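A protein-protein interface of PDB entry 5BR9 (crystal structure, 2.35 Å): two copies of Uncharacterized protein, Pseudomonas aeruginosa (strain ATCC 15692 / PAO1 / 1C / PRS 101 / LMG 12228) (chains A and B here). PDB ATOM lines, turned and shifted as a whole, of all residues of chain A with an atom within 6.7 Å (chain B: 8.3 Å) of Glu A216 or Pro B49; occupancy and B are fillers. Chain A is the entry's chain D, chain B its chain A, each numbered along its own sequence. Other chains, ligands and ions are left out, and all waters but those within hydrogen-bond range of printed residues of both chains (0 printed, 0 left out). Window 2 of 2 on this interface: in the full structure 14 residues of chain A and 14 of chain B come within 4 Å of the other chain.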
ATOM      1  N   GLN A  88       2.388  18.188  25.073  1.00  0.00           N
ATOM      2  CA  GLN A  88       2.757  17.076  25.949  1.00  0.00           C
ATOM      3  C   GLN A  88       4.081  17.331  26.677  1.00  0.00           C
ATOM      4  O   GLN A  88       4.146  17.276  27.908  1.00  0.00           O
ATOM      5  CB  GLN A  88       2.854  15.770  25.153  1.00  0.00           C
ATOM      6  CG  GLN A  88       1.529  15.084  24.939  1.00  0.00           C
ATOM      7  CD  GLN A  88       1.672  13.657  24.426  1.00  0.00           C
ATOM      8  OE1 GLN A  88       2.578  13.350  23.655  1.00  0.00           O
ATOM      9  NE2 GLN A  88       0.765  12.780  24.851  1.00  0.00           N
ATOM     10  N   PHE A  92       4.464  18.006  30.668  1.00  0.00           N
ATOM     11  CA  PHE A  92       5.197  17.002  31.422  1.00  0.00           C
ATOM     12  C   PHE A  92       6.362  17.630  32.213  1.00  0.00           C
ATOM     13  O   PHE A  92       6.521  17.391  33.411  1.00  0.00           O
ATOM     14  CB  PHE A  92       5.704  15.931  30.465  1.00  0.00           C
ATOM     15  CG  PHE A  92       6.489  14.834  31.120  1.00  0.00           C
ATOM     16  CD1 PHE A  92       5.847  13.698  31.608  1.00  0.00           C
ATOM     17  CD2 PHE A  92       7.882  14.928  31.233  1.00  0.00           C
ATOM     18  CE1 PHE A  92       6.578  12.664  32.189  1.00  0.00           C
ATOM     19  CE2 PHE A  92       8.622  13.895  31.810  1.00  0.00           C
ATOM     20  CZ  PHE A  92       7.963  12.760  32.291  1.00  0.00           C
ATOM     21  N   VAL A  98      -3.365  19.593  31.094  1.00  0.00           N
ATOM     22  CA  VAL A  98      -3.701  20.109  29.769  1.00  0.00           C
ATOM     23  C   VAL A  98      -5.219  20.155  29.586  1.00  0.00           C
ATOM     24  O   VAL A  98      -5.973  19.380  30.193  1.00  0.00           O
ATOM     25  CB  VAL A  98      -3.020  19.286  28.633  1.00  0.00           C
ATOM     26  CG1 VAL A  98      -1.524  19.164  28.903  1.00  0.00           C
ATOM     27  CG2 VAL A  98      -3.636  17.908  28.489  1.00  0.00           C
ATOM     28  N   VAL A 213      -6.437  17.325  32.387  1.00  0.00           N
ATOM     29  CA  VAL A 213      -5.907  15.952  32.409  1.00  0.00           C
ATOM     30  C   VAL A 213      -4.382  15.980  32.338  1.00  0.00           C
ATOM     31  O   VAL A 213      -3.782  17.037  32.113  1.00  0.00           O
ATOM     32  CB  VAL A 213      -6.498  15.073  31.267  1.00  0.00           C
ATOM     33  CG1 VAL A 213      -8.002  15.257  31.173  1.00  0.00           C
ATOM     34  CG2 VAL A 213      -5.830  15.352  29.919  1.00  0.00           C
ATOM     35  N   GLU A 214      -3.760  14.819  32.534  1.00  0.00           N
ATOM     36  CA  GLU A 214      -2.302  14.714  32.541  1.00  0.00           C
ATOM     37  C   GLU A 214      -1.737  14.691  31.117  1.00  0.00           C
ATOM     38  O   GLU A 214      -2.420  14.288  30.172  1.00  0.00           O
ATOM     39  CB  GLU A 214      -1.850  13.465  33.318  1.00  0.00           C
ATOM     40  N   ALA A 215      -0.491  15.136  30.985  1.00  0.00           N
ATOM     41  CA  ALA A 215       0.175  15.310  29.694  1.00  0.00           C
ATOM     42  C   ALA A 215       0.088  14.093  28.768  1.00  0.00           C
ATOM     43  O   ALA A 215      -0.076  14.244  27.560  1.00  0.00           O
ATOM     44  CB  ALA A 215       1.645  15.682  29.921  1.00  0.00           C
ATOM     45  N   GLU A 216       0.189  12.892  29.324  1.00  0.00           N
ATOM     46  CA  GLU A 216       0.147  11.686  28.501  1.00  0.00           C
ATOM     47  C   GLU A 216      -1.225  11.435  27.861  1.00  0.00           C
ATOM     48  O   GLU A 216      -1.342  10.610  26.955  1.00  0.00           O
ATOM     49  CB  GLU A 216       0.566  10.468  29.327  1.00  0.00           C
ATOM     50  CG  GLU A 216       0.021  10.450  30.743  1.00  0.00           C
ATOM     51  CD  GLU A 216       1.106  10.617  31.792  1.00  0.00           C
ATOM     52  OE1 GLU A 216       1.703  11.720  31.887  1.00  0.00           O
ATOM     53  OE2 GLU A 216       1.366   9.636  32.522  1.00  0.00           O
ATOM     54  N   GLN A 217      -2.256  12.139  28.321  1.00  0.00           N
ATOM     55  CA  GLN A 217      -3.599  11.954  27.769  1.00  0.00           C
ATOM     56  C   GLN A 217      -3.976  13.048  26.774  1.00  0.00           C
ATOM     57  O   GLN A 217      -5.093  13.068  26.261  1.00  0.00           O
ATOM     58  CB  GLN A 217      -4.639  11.903  28.880  1.00  0.00           C
ATOM     59  CG  GLN A 217      -4.273  11.018  30.055  1.00  0.00           C
ATOM     60  CD  GLN A 217      -5.286  11.148  31.176  1.00  0.00           C
ATOM     61  OE1 GLN A 217      -6.490  11.114  30.935  1.00  0.00           O
ATOM     62  NE2 GLN A 217      -4.806  11.326  32.399  1.00  0.00           N
ATOM     63  N   ALA A 218      -3.048  13.959  26.500  1.00  0.00           N
ATOM     64  CA  ALA A 218      -3.231  14.909  25.409  1.00  0.00           C
ATOM     65  C   ALA A 218      -3.162  14.170  24.078  1.00  0.00           C
ATOM     66  O   ALA A 218      -2.079  13.856  23.582  1.00  0.00           O
ATOM     67  CB  ALA A 218      -2.185  16.012  25.466  1.00  0.00           C
ATOM     68  N   LEU A 219      -4.331  13.880  23.518  1.00  0.00           N
ATOM     69  CA  LEU A 219      -4.448  13.189  22.241  1.00  0.00           C
ATOM     70  C   LEU A 219      -5.222  14.043  21.239  1.00  0.00           C
ATOM     71  O   LEU A 219      -6.108  14.812  21.628  1.00  0.00           O
ATOM     72  CB  LEU A 219      -5.158  11.843  22.414  1.00  0.00           C
ATOM     73  CG  LEU A 219      -4.359  10.610  22.829  1.00  0.00           C
ATOM     74  CD1 LEU A 219      -3.969  10.663  24.297  1.00  0.00           C
ATOM     75  CD2 LEU A 219      -5.158   9.351  22.510  1.00  0.00           C
ATOM     76  N   CYS B  22       9.144   1.553  20.937  1.00  0.00           N
ATOM     77  CA  CYS B  22       9.265   2.777  21.695  1.00  0.00           C
ATOM     78  C   CYS B  22      10.356   2.577  22.749  1.00  0.00           C
ATOM     79  O   CYS B  22      10.319   1.616  23.521  1.00  0.00           O
ATOM     80  CB  CYS B  22       7.931   3.153  22.341  1.00  0.00           C
ATOM     81  SG  CYS B  22       7.959   4.765  23.148  1.00  0.00           S
ATOM     82  N   VAL B  24      13.530   4.407  25.498  1.00  0.00           N
ATOM     83  CA  VAL B  24      14.078   5.553  26.197  1.00  0.00           C
ATOM     84  C   VAL B  24      15.373   5.122  26.871  1.00  0.00           C
ATOM     85  O   VAL B  24      15.532   3.974  27.273  1.00  0.00           O
ATOM     86  CB  VAL B  24      13.063   6.124  27.220  1.00  0.00           C
ATOM     87  CG1 VAL B  24      11.764   6.564  26.515  1.00  0.00           C
ATOM     88  CG2 VAL B  24      12.752   5.093  28.303  1.00  0.00           C
ATOM     89  N   GLU B  37      10.089  -1.148  24.330  1.00  0.00           N
ATOM     90  CA  GLU B  37       8.822  -1.869  24.176  1.00  0.00           C
ATOM     91  C   GLU B  37       8.325  -1.826  22.731  1.00  0.00           C
ATOM     92  O   GLU B  37       8.426  -0.793  22.076  1.00  0.00           O
ATOM     93  CB  GLU B  37       7.743  -1.283  25.088  1.00  0.00           C
ATOM     94  CG  GLU B  37       7.942  -1.538  26.566  1.00  0.00           C
ATOM     95  CD  GLU B  37       6.857  -0.893  27.420  1.00  0.00           C
ATOM     96  OE1 GLU B  37       5.758  -0.595  26.896  1.00  0.00           O
ATOM     97  OE2 GLU B  37       7.117  -0.672  28.619  1.00  0.00           O
ATOM     98  N   LEU B  42       0.594   3.224  19.917  1.00  0.00           N
ATOM     99  CA  LEU B  42       0.369   3.679  21.290  1.00  0.00           C
ATOM    100  C   LEU B  42       1.528   4.544  21.799  1.00  0.00           C
ATOM    101  O   LEU B  42       1.714   4.690  23.004  1.00  0.00           O
ATOM    102  CB  LEU B  42       0.149   2.481  22.223  1.00  0.00           C
ATOM    103  N   HIS B  43       2.293   5.122  20.877  1.00  0.00           N
ATOM    104  CA  HIS B  43       3.486   5.877  21.239  1.00  0.00           C
ATOM    105  C   HIS B  43       3.138   7.136  22.015  1.00  0.00           C
ATOM    106  O   HIS B  43       3.719   7.394  23.061  1.00  0.00           O
ATOM    107  CB  HIS B  43       4.298   6.253  19.998  1.00  0.00           C
ATOM    108  CG  HIS B  43       4.904   5.080  19.291  1.00  0.00           C
ATOM    109  ND1 HIS B  43       6.093   4.508  19.684  1.00  0.00           N
ATOM    110  CD2 HIS B  43       4.488   4.377  18.210  1.00  0.00           C
ATOM    111  CE1 HIS B  43       6.383   3.502  18.879  1.00  0.00           C
ATOM    112  NE2 HIS B  43       5.426   3.402  17.976  1.00  0.00           N
ATOM    113  N   ALA B  44       2.183   7.903  21.498  1.00  0.00           N
ATOM    114  CA  ALA B  44       1.775   9.181  22.089  1.00  0.00           C
ATOM    115  C   ALA B  44       1.247   9.033  23.517  1.00  0.00           C
ATOM    116  O   ALA B  44       1.198  10.004  24.278  1.00  0.00           O
ATOM    117  CB  ALA B  44       0.715   9.853  21.215  1.00  0.00           C
ATOM    118  N   GLN B  45       0.841   7.820  23.871  1.00  0.00           N
ATOM    119  CA  GLN B  45       0.307   7.581  25.195  1.00  0.00           C
ATOM    120  C   GLN B  45       1.326   6.905  26.085  1.00  0.00           C
ATOM    121  O   GLN B  45       1.189   6.922  27.303  1.00  0.00           O
ATOM    122  CB  GLN B  45      -0.959   6.734  25.116  1.00  0.00           C
ATOM    123  CG  GLN B  45      -2.047   7.340  24.277  1.00  0.00           C
ATOM    124  CD  GLN B  45      -2.529   6.368  23.236  1.00  0.00           C
ATOM    125  OE1 GLN B  45      -2.014   6.336  22.114  1.00  0.00           O
ATOM    126  NE2 GLN B  45      -3.505   5.544  23.606  1.00  0.00           N
ATOM    127  N   ARG B  46       2.352   6.308  25.487  1.00  0.00           N
ATOM    128  CA  ARG B  46       3.261   5.501  26.281  1.00  0.00           C
ATOM    129  C   ARG B  46       4.653   6.102  26.425  1.00  0.00           C
ATOM    130  O   ARG B  46       5.408   5.669  27.284  1.00  0.00           O
ATOM    131  CB  ARG B  46       3.345   4.091  25.702  1.00  0.00           C
ATOM    132  CG  ARG B  46       2.199   3.197  26.176  1.00  0.00           C
ATOM    133  CD  ARG B  46       2.694   1.991  26.990  1.00  0.00           C
ATOM    134  NE  ARG B  46       3.860   2.285  27.834  1.00  0.00           N
ATOM    135  CZ  ARG B  46       3.806   2.684  29.108  1.00  0.00           C
ATOM    136  NH1 ARG B  46       2.632   2.855  29.716  1.00  0.00           N
ATOM    137  NH2 ARG B  46       4.932   2.914  29.785  1.00  0.00           N
ATOM    138  N   LEU B  47       4.984   7.105  25.614  1.00  0.00           N
ATOM    139  CA  LEU B  47       6.323   7.681  25.639  1.00  0.00           C
ATOM    140  C   LEU B  47       6.657   8.372  26.966  1.00  0.00           C
ATOM    141  O   LEU B  47       7.672   8.066  27.594  1.00  0.00           O
ATOM    142  CB  LEU B  47       6.506   8.676  24.493  1.00  0.00           C
ATOM    143  CG  LEU B  47       7.888   9.335  24.461  1.00  0.00           C
ATOM    144  CD1 LEU B  47       8.940   8.259  24.326  1.00  0.00           C
ATOM    145  CD2 LEU B  47       7.992  10.312  23.293  1.00  0.00           C
ATOM    146  N   LEU B  48       5.821   9.317  27.384  1.00  0.00           N
ATOM    147  CA  LEU B  48       6.098  10.056  28.614  1.00  0.00           C
ATOM    148  C   LEU B  48       6.044   9.184  29.877  1.00  0.00           C
ATOM    149  O   LEU B  48       6.817   9.405  30.798  1.00  0.00           O
ATOM    150  CB  LEU B  48       5.152  11.243  28.746  1.00  0.00           C
ATOM    151  CG  LEU B  48       5.475  12.324  27.703  1.00  0.00           C
ATOM    152  CD1 LEU B  48       4.542  13.526  27.867  1.00  0.00           C
ATOM    153  CD2 LEU B  48       6.951  12.744  27.731  1.00  0.00           C
ATOM    154  N   PRO B  49       5.115   8.220  29.956  1.00  0.00           N
ATOM    155  CA  PRO B  49       5.260   7.357  31.136  1.00  0.00           C
ATOM    156  C   PRO B  49       6.554   6.523  31.125  1.00  0.00           C
ATOM    157  O   PRO B  49       7.109   6.243  32.194  1.00  0.00           O
ATOM    158  CB  PRO B  49       4.017   6.454  31.075  1.00  0.00           C
ATOM    159  CG  PRO B  49       3.013   7.243  30.281  1.00  0.00           C
ATOM    160  CD  PRO B  49       3.817   8.033  29.280  1.00  0.00           C
ATOM    161  N   MET B  50       7.033   6.123  29.952  1.00  0.00           N
ATOM    162  CA  MET B  50       8.302   5.398  29.909  1.00  0.00           C
ATOM    163  C   MET B  50       9.430   6.280  30.444  1.00  0.00           C
ATOM    164  O   MET B  50      10.319   5.802  31.151  1.00  0.00           O
ATOM    165  CB  MET B  50       8.623   4.916  28.501  1.00  0.00           C
ATOM    166  CG  MET B  50       7.875   3.651  28.108  1.00  0.00           C
ATOM    167  SD  MET B  50       8.375   3.011  26.492  1.00  0.00           S
ATOM    168  CE  MET B  50      10.125   2.870  26.757  1.00  0.00           C
ATOM    169  N   VAL B  51       9.370   7.569  30.120  1.00  0.00           N
ATOM    170  CA  VAL B  51      10.366   8.528  30.574  1.00  0.00           C
ATOM    171  C   VAL B  51      10.298   8.717  32.081  1.00  0.00           C
ATOM    172  O   VAL B  51      11.337   8.685  32.765  1.00  0.00           O
ATOM    173  CB  VAL B  51      10.209   9.870  29.848  1.00  0.00           C
ATOM    174  CG1 VAL B  51      11.096  10.941  30.500  1.00  0.00           C
ATOM    175  CG2 VAL B  51      10.579   9.702  28.364  1.00  0.00           C
ATOM    176  N   ARG B  52       9.082   8.901  32.602  1.00  0.00           N
ATOM    177  CA  ARG B  52       8.901   9.083  34.037  1.00  0.00           C
ATOM    178  C   ARG B  52       9.484   7.873  34.769  1.00  0.00           C
ATOM    179  O   ARG B  52      10.251   8.025  35.720  1.00  0.00           O
ATOM    180  CB  ARG B  52       7.413   9.293  34.366  1.00  0.00           C
ATOM    181  CG  ARG B  52       7.021   9.342  35.850  1.00  0.00           C
ATOM    182  CD  ARG B  52       7.925  10.240  36.704  1.00  0.00           C
ATOM    183  NE  ARG B  52       8.147  11.574  36.151  1.00  0.00           N
ATOM    184  CZ  ARG B  52       9.149  12.359  36.525  1.00  0.00           C
ATOM    185  NH1 ARG B  52       9.998  11.922  37.439  1.00  0.00           N
ATOM    186  NH2 ARG B  52       9.310  13.562  35.989  1.00  0.00           N
ATOM    187  N   ASP B  53       9.133   6.677  34.303  1.00  0.00           N
ATOM    188  CA  ASP B  53       9.589   5.436  34.939  1.00  0.00           C
ATOM    189  C   ASP B  53      11.108   5.295  34.917  1.00  0.00           C
ATOM    190  O   ASP B  53      11.710   4.845  35.896  1.00  0.00           O
ATOM    191  CB  ASP B  53       8.960   4.212  34.263  1.00  0.00           C
ATOM    192  CG  ASP B  53       7.479   4.047  34.586  1.00  0.00           C
ATOM    193  OD1 ASP B  53       6.948   4.782  35.453  1.00  0.00           O
ATOM    194  OD2 ASP B  53       6.842   3.179  33.951  1.00  0.00           O
ATOM    195  N   LEU B  54      11.715   5.655  33.793  1.00  0.00           N
ATOM    196  CA  LEU B  54      13.158   5.545  33.637  1.00  0.00           C
ATOM    197  C   LEU B  54      13.860   6.502  34.604  1.00  0.00           C
ATOM    198  O   LEU B  54      14.774   6.112  35.344  1.00  0.00           O
ATOM    199  CB  LEU B  54      13.571   5.851  32.200  1.00  0.00           C
ATOM    200  CG  LEU B  54      15.063   5.709  31.883  1.00  0.00           C
ATOM    201  CD1 LEU B  54      15.476   4.253  31.915  1.00  0.00           C
ATOM    202  CD2 LEU B  54      15.404   6.317  30.528  1.00  0.00           C
ATOM    203  N   LEU B  55      13.424   7.755  34.595  1.00  0.00           N
ATOM    204  CA  LEU B  55      13.985   8.746  35.499  1.00  0.00           C
ATOM    205  C   LEU B  55      13.762   8.300  36.933  1.00  0.00           C
ATOM    206  O   LEU B  55      14.670   8.362  37.756  1.00  0.00           O
ATOM    207  CB  LEU B  55      13.359  10.117  35.279  1.00  0.00           C
ATOM    208  CG  LEU B  55      13.680  10.822  33.970  1.00  0.00           C
ATOM    209  CD1 LEU B  55      12.819  12.064  33.902  1.00  0.00           C
ATOM    210  CD2 LEU B  55      15.143  11.189  33.914  1.00  0.00           C
ATOM    211  N   ASP B  56      12.572   7.795  37.222  1.00  0.00           N
ATOM    212  CA  ASP B  56      12.275   7.385  38.594  1.00  0.00           C
ATOM    213  C   ASP B  56      13.103   6.178  39.025  1.00  0.00           C
ATOM    214  O   ASP B  56      13.567   6.130  40.155  1.00  0.00           O
ATOM    215  CB  ASP B  56      10.780   7.103  38.763  1.00  0.00           C
ATOM    216  CG  ASP B  56       9.958   8.382  38.851  1.00  0.00           C
ATOM    217  OD1 ASP B  56      10.540   9.495  38.705  1.00  0.00           O
ATOM    218  OD2 ASP B  56       8.734   8.275  39.083  1.00  0.00           O
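Of the 18 printed residues of chain B, 4 touch a printed residue of chain A.
Printed residues of chain B that touch a printed residue of chain A: Ala B44, Gln B45, Leu B48 and Pro B49.
Along chain B the printed residues that touch a printed residue of chain A span positions 44 to 49.
Hydrophobic or aromatic side chains of chain A that line the printed part of chain B: Phe A92 and Leu A219.
Among the printed residues, no Asp or Glu carboxylate lies within 4 Å of a Lys or Arg side-chain nitrogen of the other chain.
Among the printed residues, pairs that only touch across the chains: Phe A92 with Leu B48 (3.6 Å), Glu A216 with Pro B49 (3.7 Å), Glu A216 with Ala B44 (3.7 Å), Gln A88 with Leu B48 (3.8 Å), Leu A219 with Gln B45 (3.8 Å) and Glu A216 with Gln B45 (3.9 Å).
The side-chain amide nitrogen (NE2) of Gln A88 sits close to the backbone carbonyl oxygen (O) of Ala A215 (3.2 Å).
The backbone carbonyl oxygen (O) of Ala A218 is in hydrogen-bond range of the side-chain amide nitrogen (NE2) of Gln A88, at 3.3 Å.
No position is printed for both chains.
Of the 7 pairs that touch across the chains among the printed residues, none has its exchanged pair printed and touching as well.
O of Ala B44 lies within hydrogen-bond range of NE2 of Gln A88 (2.9 Å).
Pro B49 touches one residue of chain A.
No residue of chain B comes within 4 Å of Ala A215.
Of the printed residues of chain B, Leu A219 touches Gln B45.
Printed residues of chain A within 4 Å of Ala B44: Gln A88 (2.9 Å) and Glu A216 (3.7 Å).
Of the printed residues of chain B, Gln A88 touches Ala B44 and Leu B48.
Val B51 touches none of the printed residues of chain A.
Leu B42 touches none of the printed residues of chain A.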
